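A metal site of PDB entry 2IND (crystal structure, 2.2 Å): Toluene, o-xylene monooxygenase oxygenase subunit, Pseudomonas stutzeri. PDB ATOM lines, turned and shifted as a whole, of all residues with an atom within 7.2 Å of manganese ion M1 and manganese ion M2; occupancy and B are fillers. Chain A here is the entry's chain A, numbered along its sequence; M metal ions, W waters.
The backbone carbonyl oxygen (O) of Leu 191 is in hydrogen-bond range of the backbone NH (N) of Glu 196, 2.9 Å away. The backbone carbonyl oxygen of Glu 196 sits close to the side-chain hydroxyl of Thr 200 (3.4 Å). The backbone NH (N) of Asn 201 is in hydrogen-bond range of the backbone carbonyl oxygen (O) of Glu 196. O of His 136 lies close to NE2 of Gln 140. A ring nitrogen (NE2) of His 136 lies within hydrogen-bond range of the side-chain carboxylate of Asp 229 (2.9 Å). The side-chain carboxylate (OE1) of Glu 103 lies within hydrogen-bond range of the side-chain amide nitrogen (NE2) of Gln 140 (3.0 Å). OD2 of Asp 132 sits at hydrogen-bond distance from ND1 of His 233. The backbone carbonyl oxygen (O) of Asp 229 lies within hydrogen-bond range of a ring nitrogen (ND1) of His 233, 3.3 Å away.
Within 4 Å of manganese ion M1: Glu 103, Glu 133, His 136 and Glu 230.
Within 4 Å of manganese ion M2: Glu 133, Glu 196, Glu 230 and His 233.
Water W1 is bound to manganese ion M1 (2.1 Å). Manganese ion M1 is bound by OE2 of Glu 133 (2.1 Å). ND1 of His 136 binds manganese ion M1 (2.2 Å). Manganese ion M1 is bound by the side-chain carboxylate (OE2) of Glu 103 (2.3 Å). OE1 of Glu 230 binds manganese ion M1 (2.3 Å). Manganese ion M1 has five donor atoms within binding distance. Slightly farther from manganese ion M1 lies water W2 (2.8 Å).
Manganese ion M2 is bound by the side-chain carboxylate (OE2) of Glu 196, 2.0 Å away. OE2 of Glu 230 binds manganese ion M2, 2.2 Å away. Manganese ion M2 is bound by water W2 (2.2 Å). NE2 of His 233 is bound to manganese ion M2 (2.3 Å). Manganese ion M2 is bound by OE1 of Glu 133, 2.3 Å away. Manganese ion M2 is bound by OE1 of Glu 230, 2.3 Å away.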
ATOM      1  N   GLU A 102     -18.951  11.621  34.688  1.00  0.00           N
ATOM      2  CA  GLU A 102     -19.137  10.373  33.939  1.00  0.00           C
ATOM      3  C   GLU A 102     -18.706  10.678  32.496  1.00  0.00           C
ATOM      4  O   GLU A 102     -18.177   9.826  31.801  1.00  0.00           O
ATOM      5  CB  GLU A 102     -20.596   9.899  34.036  1.00  0.00           C
ATOM      6  CG  GLU A 102     -21.005   9.456  35.455  1.00  0.00           C
ATOM      7  CD  GLU A 102     -20.287   8.188  35.928  1.00  0.00           C
ATOM      8  OE1 GLU A 102     -19.192   7.882  35.433  1.00  0.00           O
ATOM      9  OE2 GLU A 102     -20.817   7.495  36.821  1.00  0.00           O
ATOM     10  N   GLU A 103     -18.899  11.922  32.060  1.00  0.00           N
ATOM     11  CA  GLU A 103     -18.448  12.316  30.722  1.00  0.00           C
ATOM     12  C   GLU A 103     -16.930  12.124  30.678  1.00  0.00           C
ATOM     13  O   GLU A 103     -16.376  11.543  29.728  1.00  0.00           O
ATOM     14  CB  GLU A 103     -18.781  13.783  30.443  1.00  0.00           C
ATOM     15  CG  GLU A 103     -20.256  14.083  30.170  1.00  0.00           C
ATOM     16  CD  GLU A 103     -20.664  13.771  28.730  1.00  0.00           C
ATOM     17  OE1 GLU A 103     -21.702  14.284  28.281  1.00  0.00           O
ATOM     18  OE2 GLU A 103     -19.943  12.993  28.072  1.00  0.00           O
ATOM     19  N   TYR A 104     -16.249  12.624  31.711  1.00  0.00           N
ATOM     20  CA  TYR A 104     -14.796  12.531  31.794  1.00  0.00           C
ATOM     21  C   TYR A 104     -14.331  11.082  31.869  1.00  0.00           C
ATOM     22  O   TYR A 104     -13.324  10.699  31.293  1.00  0.00           O
ATOM     23  CB  TYR A 104     -14.266  13.300  33.010  1.00  0.00           C
ATOM     24  CG  TYR A 104     -12.752  13.292  33.097  1.00  0.00           C
ATOM     25  CD1 TYR A 104     -11.972  14.039  32.220  1.00  0.00           C
ATOM     26  CD2 TYR A 104     -12.099  12.510  34.039  1.00  0.00           C
ATOM     27  CE1 TYR A 104     -10.574  14.008  32.269  1.00  0.00           C
ATOM     28  CE2 TYR A 104     -10.702  12.463  34.110  1.00  0.00           C
ATOM     29  CZ  TYR A 104      -9.944  13.209  33.213  1.00  0.00           C
ATOM     30  OH  TYR A 104      -8.566  13.139  33.275  1.00  0.00           O
ATOM     31  N   ALA A 106     -15.786   8.638  30.564  1.00  0.00           N
ATOM     32  CA  ALA A 106     -15.987   8.049  29.231  1.00  0.00           C
ATOM     33  C   ALA A 106     -14.739   8.173  28.358  1.00  0.00           C
ATOM     34  O   ALA A 106     -14.567   7.376  27.416  1.00  0.00           O
ATOM     35  CB  ALA A 106     -17.182   8.711  28.543  1.00  0.00           C
ATOM     36  N   GLU A 110     -13.121   5.306  26.206  1.00  0.00           N
ATOM     37  CA  GLU A 110     -12.704   5.444  24.821  1.00  0.00           C
ATOM     38  C   GLU A 110     -11.256   5.006  24.675  1.00  0.00           C
ATOM     39  O   GLU A 110     -10.888   4.304  23.723  1.00  0.00           O
ATOM     40  CB  GLU A 110     -12.874   6.894  24.357  1.00  0.00           C
ATOM     41  CG  GLU A 110     -14.313   7.321  24.077  1.00  0.00           C
ATOM     42  CD  GLU A 110     -14.888   6.783  22.751  1.00  0.00           C
ATOM     43  OE1 GLU A 110     -14.110   6.339  21.879  1.00  0.00           O
ATOM     44  OE2 GLU A 110     -16.134   6.824  22.582  1.00  0.00           O
ATOM     45  N   GLY A 129     -12.825  10.041  19.979  1.00  0.00           N
ATOM     46  CA  GLY A 129     -13.915   9.988  20.940  1.00  0.00           C
ATOM     47  C   GLY A 129     -13.384  10.306  22.327  1.00  0.00           C
ATOM     48  O   GLY A 129     -14.060  10.938  23.168  1.00  0.00           O
ATOM     49  N   ASP A 132     -13.268  13.807  22.581  1.00  0.00           N
ATOM     50  CA  ASP A 132     -14.605  14.389  22.708  1.00  0.00           C
ATOM     51  C   ASP A 132     -15.091  14.400  24.159  1.00  0.00           C
ATOM     52  O   ASP A 132     -15.616  15.400  24.647  1.00  0.00           O
ATOM     53  CB  ASP A 132     -15.668  13.613  21.885  1.00  0.00           C
ATOM     54  CG  ASP A 132     -15.469  13.735  20.373  1.00  0.00           C
ATOM     55  OD1 ASP A 132     -14.925  14.756  19.902  1.00  0.00           O
ATOM     56  OD2 ASP A 132     -15.906  12.807  19.662  1.00  0.00           O
ATOM     57  N   GLU A 133     -14.936  13.272  24.843  1.00  0.00           N
ATOM     58  CA  GLU A 133     -15.390  13.167  26.215  1.00  0.00           C
ATOM     59  C   GLU A 133     -14.520  14.017  27.141  1.00  0.00           C
ATOM     60  O   GLU A 133     -14.955  14.416  28.223  1.00  0.00           O
ATOM     61  CB  GLU A 133     -15.357  11.703  26.664  1.00  0.00           C
ATOM     62  CG  GLU A 133     -15.977  10.704  25.669  1.00  0.00           C
ATOM     63  CD  GLU A 133     -17.490  10.746  25.590  1.00  0.00           C
ATOM     64  OE1 GLU A 133     -18.076   9.672  25.350  1.00  0.00           O
ATOM     65  OE2 GLU A 133     -18.114  11.826  25.751  1.00  0.00           O
ATOM     66  N   ASN A 134     -13.292  14.290  26.729  1.00  0.00           N
ATOM     67  CA  ASN A 134     -12.407  15.128  27.530  1.00  0.00           C
ATOM     68  C   ASN A 134     -13.066  16.517  27.472  1.00  0.00           C
ATOM     69  O   ASN A 134     -13.201  17.200  28.490  1.00  0.00           O
ATOM     70  CB  ASN A 134     -10.986  15.137  26.932  1.00  0.00           C
ATOM     71  CG  ASN A 134     -10.056  16.114  27.628  1.00  0.00           C
ATOM     72  OD1 ASN A 134      -9.936  17.274  27.220  1.00  0.00           O
ATOM     73  ND2 ASN A 134      -9.397  15.662  28.688  1.00  0.00           N
ATOM     74  N   ARG A 135     -13.511  16.894  26.274  1.00  0.00           N
ATOM     75  CA  ARG A 135     -14.184  18.178  26.073  1.00  0.00           C
ATOM     76  C   ARG A 135     -15.473  18.243  26.885  1.00  0.00           C
ATOM     77  O   ARG A 135     -15.747  19.223  27.589  1.00  0.00           O
ATOM     78  CB  ARG A 135     -14.539  18.378  24.591  1.00  0.00           C
ATOM     79  CG  ARG A 135     -15.272  19.700  24.319  1.00  0.00           C
ATOM     80  CD  ARG A 135     -15.975  19.716  22.976  1.00  0.00           C
ATOM     81  NE  ARG A 135     -16.550  21.033  22.706  1.00  0.00           N
ATOM     82  CZ  ARG A 135     -17.685  21.249  22.026  1.00  0.00           C
ATOM     83  NH1 ARG A 135     -18.390  20.226  21.545  1.00  0.00           N
ATOM     84  NH2 ARG A 135     -18.118  22.484  21.851  1.00  0.00           N
ATOM     85  N   HIS A 136     -16.275  17.193  26.771  1.00  0.00           N
ATOM     86  CA  HIS A 136     -17.554  17.117  27.465  1.00  0.00           C
ATOM     87  C   HIS A 136     -17.399  17.191  28.981  1.00  0.00           C
ATOM     88  O   HIS A 136     -18.160  17.861  29.661  1.00  0.00           O
ATOM     89  CB  HIS A 136     -18.281  15.834  27.043  1.00  0.00           C
ATOM     90  CG  HIS A 136     -18.559  15.777  25.571  1.00  0.00           C
ATOM     91  ND1 HIS A 136     -19.200  14.727  24.964  1.00  0.00           N
ATOM     92  CD2 HIS A 136     -18.265  16.669  24.582  1.00  0.00           C
ATOM     93  CE1 HIS A 136     -19.298  14.962  23.662  1.00  0.00           C
ATOM     94  NE2 HIS A 136     -18.740  16.130  23.411  1.00  0.00           N
ATOM     95  N   GLY A 137     -16.401  16.504  29.518  1.00  0.00           N
ATOM     96  CA  GLY A 137     -16.202  16.572  30.950  1.00  0.00           C
ATOM     97  C   GLY A 137     -15.794  17.980  31.350  1.00  0.00           C
ATOM     98  O   GLY A 137     -16.324  18.533  32.315  1.00  0.00           O
ATOM     99  N   GLN A 140     -18.577  20.826  30.705  1.00  0.00           N
ATOM    100  CA  GLN A 140     -19.712  20.703  31.610  1.00  0.00           C
ATOM    101  C   GLN A 140     -19.318  20.911  33.068  1.00  0.00           C
ATOM    102  O   GLN A 140     -20.082  20.597  34.001  1.00  0.00           O
ATOM    103  CB  GLN A 140     -20.439  19.382  31.381  1.00  0.00           C
ATOM    104  CG  GLN A 140     -20.902  19.336  29.938  1.00  0.00           C
ATOM    105  CD  GLN A 140     -21.903  18.250  29.655  1.00  0.00           C
ATOM    106  OE1 GLN A 140     -23.111  18.467  29.774  1.00  0.00           O
ATOM    107  NE2 GLN A 140     -21.414  17.067  29.284  1.00  0.00           N
ATOM    108  N   LEU A 191     -21.719   0.773  25.190  1.00  0.00           N
ATOM    109  CA  LEU A 191     -21.686   2.226  25.351  1.00  0.00           C
ATOM    110  C   LEU A 191     -22.059   3.052  24.125  1.00  0.00           C
ATOM    111  O   LEU A 191     -23.060   3.770  24.147  1.00  0.00           O
ATOM    112  CB  LEU A 191     -20.302   2.670  25.843  1.00  0.00           C
ATOM    113  CG  LEU A 191     -20.058   4.189  25.893  1.00  0.00           C
ATOM    114  CD1 LEU A 191     -21.004   4.842  26.892  1.00  0.00           C
ATOM    115  CD2 LEU A 191     -18.597   4.462  26.266  1.00  0.00           C
ATOM    116  N   THR A 192     -21.282   2.970  23.049  1.00  0.00           N
ATOM    117  CA  THR A 192     -21.566   3.772  21.870  1.00  0.00           C
ATOM    118  C   THR A 192     -22.828   3.394  21.123  1.00  0.00           C
ATOM    119  O   THR A 192     -23.567   4.265  20.665  1.00  0.00           O
ATOM    120  CB  THR A 192     -20.358   3.792  20.872  1.00  0.00           C
ATOM    121  OG1 THR A 192     -20.136   2.477  20.345  1.00  0.00           O
ATOM    122  CG2 THR A 192     -19.084   4.284  21.574  1.00  0.00           C
ATOM    123  N   PHE A 195     -26.110   2.811  24.533  1.00  0.00           N
ATOM    124  CA  PHE A 195     -26.400   4.042  25.278  1.00  0.00           C
ATOM    125  C   PHE A 195     -26.370   5.352  24.501  1.00  0.00           C
ATOM    126  O   PHE A 195     -27.309   6.147  24.592  1.00  0.00           O
ATOM    127  CB  PHE A 195     -25.460   4.141  26.478  1.00  0.00           C
ATOM    128  CG  PHE A 195     -25.738   5.328  27.359  1.00  0.00           C
ATOM    129  CD1 PHE A 195     -26.914   5.385  28.106  1.00  0.00           C
ATOM    130  CD2 PHE A 195     -24.824   6.370  27.461  1.00  0.00           C
ATOM    131  CE1 PHE A 195     -27.173   6.479  28.943  1.00  0.00           C
ATOM    132  CE2 PHE A 195     -25.065   7.465  28.301  1.00  0.00           C
ATOM    133  CZ  PHE A 195     -26.239   7.517  29.035  1.00  0.00           C
ATOM    134  N   GLU A 196     -25.310   5.592  23.745  1.00  0.00           N
ATOM    135  CA  GLU A 196     -25.203   6.848  23.009  1.00  0.00           C
ATOM    136  C   GLU A 196     -26.089   6.903  21.769  1.00  0.00           C
ATOM    137  O   GLU A 196     -26.981   7.742  21.656  1.00  0.00           O
ATOM    138  CB  GLU A 196     -23.736   7.101  22.627  1.00  0.00           C
ATOM    139  CG  GLU A 196     -22.801   7.234  23.843  1.00  0.00           C
ATOM    140  CD  GLU A 196     -21.320   7.272  23.466  1.00  0.00           C
ATOM    141  OE1 GLU A 196     -20.923   6.510  22.567  1.00  0.00           O
ATOM    142  OE2 GLU A 196     -20.554   8.048  24.081  1.00  0.00           O
ATOM    143  N   THR A 200     -28.873   8.771  24.404  1.00  0.00           N
ATOM    144  CA  THR A 200     -28.365  10.139  24.518  1.00  0.00           C
ATOM    145  C   THR A 200     -28.281  10.985  23.254  1.00  0.00           C
ATOM    146  O   THR A 200     -28.436  12.207  23.319  1.00  0.00           O
ATOM    147  CB  THR A 200     -26.982  10.129  25.205  1.00  0.00           C
ATOM    148  OG1 THR A 200     -26.030   9.439  24.392  1.00  0.00           O
ATOM    149  CG2 THR A 200     -27.093   9.423  26.532  1.00  0.00           C
ATOM    150  N   ASN A 201     -28.044  10.350  22.107  1.00  0.00           N
ATOM    151  CA  ASN A 201     -27.964  11.100  20.859  1.00  0.00           C
ATOM    152  C   ASN A 201     -29.245  11.908  20.653  1.00  0.00           C
ATOM    153  O   ASN A 201     -29.211  13.083  20.280  1.00  0.00           O
ATOM    154  CB  ASN A 201     -27.750  10.152  19.676  1.00  0.00           C
ATOM    155  CG  ASN A 201     -26.274   9.997  19.294  1.00  0.00           C
ATOM    156  OD1 ASN A 201     -25.369  10.295  20.074  1.00  0.00           O
ATOM    157  ND2 ASN A 201     -26.037   9.521  18.074  1.00  0.00           N
ATOM    158  N   PHE A 204     -30.267  14.400  24.056  1.00  0.00           N
ATOM    159  CA  PHE A 204     -29.593  15.693  24.003  1.00  0.00           C
ATOM    160  C   PHE A 204     -30.230  16.627  23.001  1.00  0.00           C
ATOM    161  O   PHE A 204     -30.185  17.845  23.161  1.00  0.00           O
ATOM    162  CB  PHE A 204     -28.116  15.490  23.664  1.00  0.00           C
ATOM    163  CG  PHE A 204     -27.224  15.353  24.877  1.00  0.00           C
ATOM    164  CD1 PHE A 204     -27.625  14.600  25.978  1.00  0.00           C
ATOM    165  CD2 PHE A 204     -25.988  15.980  24.915  1.00  0.00           C
ATOM    166  CE1 PHE A 204     -26.807  14.480  27.103  1.00  0.00           C
ATOM    167  CE2 PHE A 204     -25.162  15.862  26.033  1.00  0.00           C
ATOM    168  CZ  PHE A 204     -25.570  15.116  27.129  1.00  0.00           C
ATOM    169  N   ILE A 226     -22.295  19.704  22.099  1.00  0.00           N
ATOM    170  CA  ILE A 226     -21.874  18.400  22.587  1.00  0.00           C
ATOM    171  C   ILE A 226     -22.488  17.306  21.725  1.00  0.00           C
ATOM    172  O   ILE A 226     -21.838  16.334  21.353  1.00  0.00           O
ATOM    173  CB  ILE A 226     -22.336  18.162  24.045  1.00  0.00           C
ATOM    174  CG1 ILE A 226     -21.752  19.229  24.983  1.00  0.00           C
ATOM    175  CG2 ILE A 226     -21.939  16.780  24.507  1.00  0.00           C
ATOM    176  CD1 ILE A 226     -20.259  19.292  24.946  1.00  0.00           C
ATOM    177  N   ASP A 229     -20.724  16.116  18.600  1.00  0.00           N
ATOM    178  CA  ASP A 229     -19.545  15.267  18.814  1.00  0.00           C
ATOM    179  C   ASP A 229     -19.995  13.815  19.030  1.00  0.00           C
ATOM    180  O   ASP A 229     -19.374  12.885  18.520  1.00  0.00           O
ATOM    181  CB  ASP A 229     -18.740  15.690  20.061  1.00  0.00           C
ATOM    182  CG  ASP A 229     -18.234  17.125  19.985  1.00  0.00           C
ATOM    183  OD1 ASP A 229     -18.121  17.676  18.870  1.00  0.00           O
ATOM    184  OD2 ASP A 229     -17.926  17.693  21.057  1.00  0.00           O
ATOM    185  N   GLU A 230     -21.043  13.650  19.826  1.00  0.00           N
ATOM    186  CA  GLU A 230     -21.596  12.344  20.158  1.00  0.00           C
ATOM    187  C   GLU A 230     -22.080  11.635  18.901  1.00  0.00           C
ATOM    188  O   GLU A 230     -21.825  10.450  18.689  1.00  0.00           O
ATOM    189  CB  GLU A 230     -22.777  12.502  21.126  1.00  0.00           C
ATOM    190  CG  GLU A 230     -22.408  12.950  22.535  1.00  0.00           C
ATOM    191  CD  GLU A 230     -21.544  11.932  23.258  1.00  0.00           C
ATOM    192  OE1 GLU A 230     -20.392  12.273  23.618  1.00  0.00           O
ATOM    193  OE2 GLU A 230     -21.999  10.796  23.458  1.00  0.00           O
ATOM    194  N   SER A 231     -22.790  12.389  18.079  1.00  0.00           N
ATOM    195  CA  SER A 231     -23.325  11.897  16.826  1.00  0.00           C
ATOM    196  C   SER A 231     -22.198  11.292  15.996  1.00  0.00           C
ATOM    197  O   SER A 231     -22.428  10.440  15.146  1.00  0.00           O
ATOM    198  CB  SER A 231     -23.988  13.056  16.067  1.00  0.00           C
ATOM    199  OG  SER A 231     -24.446  12.647  14.790  1.00  0.00           O
ATOM    200  N   HIS A 233     -18.739  10.023  17.367  1.00  0.00           N
ATOM    201  CA  HIS A 233     -18.111   8.832  17.940  1.00  0.00           C
ATOM    202  C   HIS A 233     -19.049   7.707  18.378  1.00  0.00           C
ATOM    203  O   HIS A 233     -18.601   6.603  18.664  1.00  0.00           O
ATOM    204  CB  HIS A 233     -17.163   9.195  19.110  1.00  0.00           C
ATOM    205  CG  HIS A 233     -17.850   9.758  20.317  1.00  0.00           C
ATOM    206  ND1 HIS A 233     -17.723  11.080  20.694  1.00  0.00           N
ATOM    207  CD2 HIS A 233     -18.640   9.176  21.249  1.00  0.00           C
ATOM    208  CE1 HIS A 233     -18.399  11.284  21.805  1.00  0.00           C
ATOM    209  NE2 HIS A 233     -18.960  10.145  22.167  1.00  0.00           N
ATOM    210  N   ALA A 234     -20.343   7.995  18.424  1.00  0.00           N
ATOM    211  CA  ALA A 234     -21.329   6.991  18.820  1.00  0.00           C
ATOM    212  C   ALA A 234     -21.419   5.852  17.802  1.00  0.00           C
ATOM    213  O   ALA A 234     -21.946   4.796  18.104  1.00  0.00           O
ATOM    214  CB  ALA A 234     -22.700   7.644  18.974  1.00  0.00           C
HETATM  215 MN    MN M   1     -19.939  12.878  25.810  1.00  0.00          MN
HETATM  216 MN    MN M   2     -20.071  10.029  24.201  1.00  0.00          MN
HETATM  217  O   HOH W   1     -21.913  13.532  25.932  1.00  0.00           O
HETATM  218  O   HOH W   2     -20.919  10.330  26.235  1.00  0.00           O
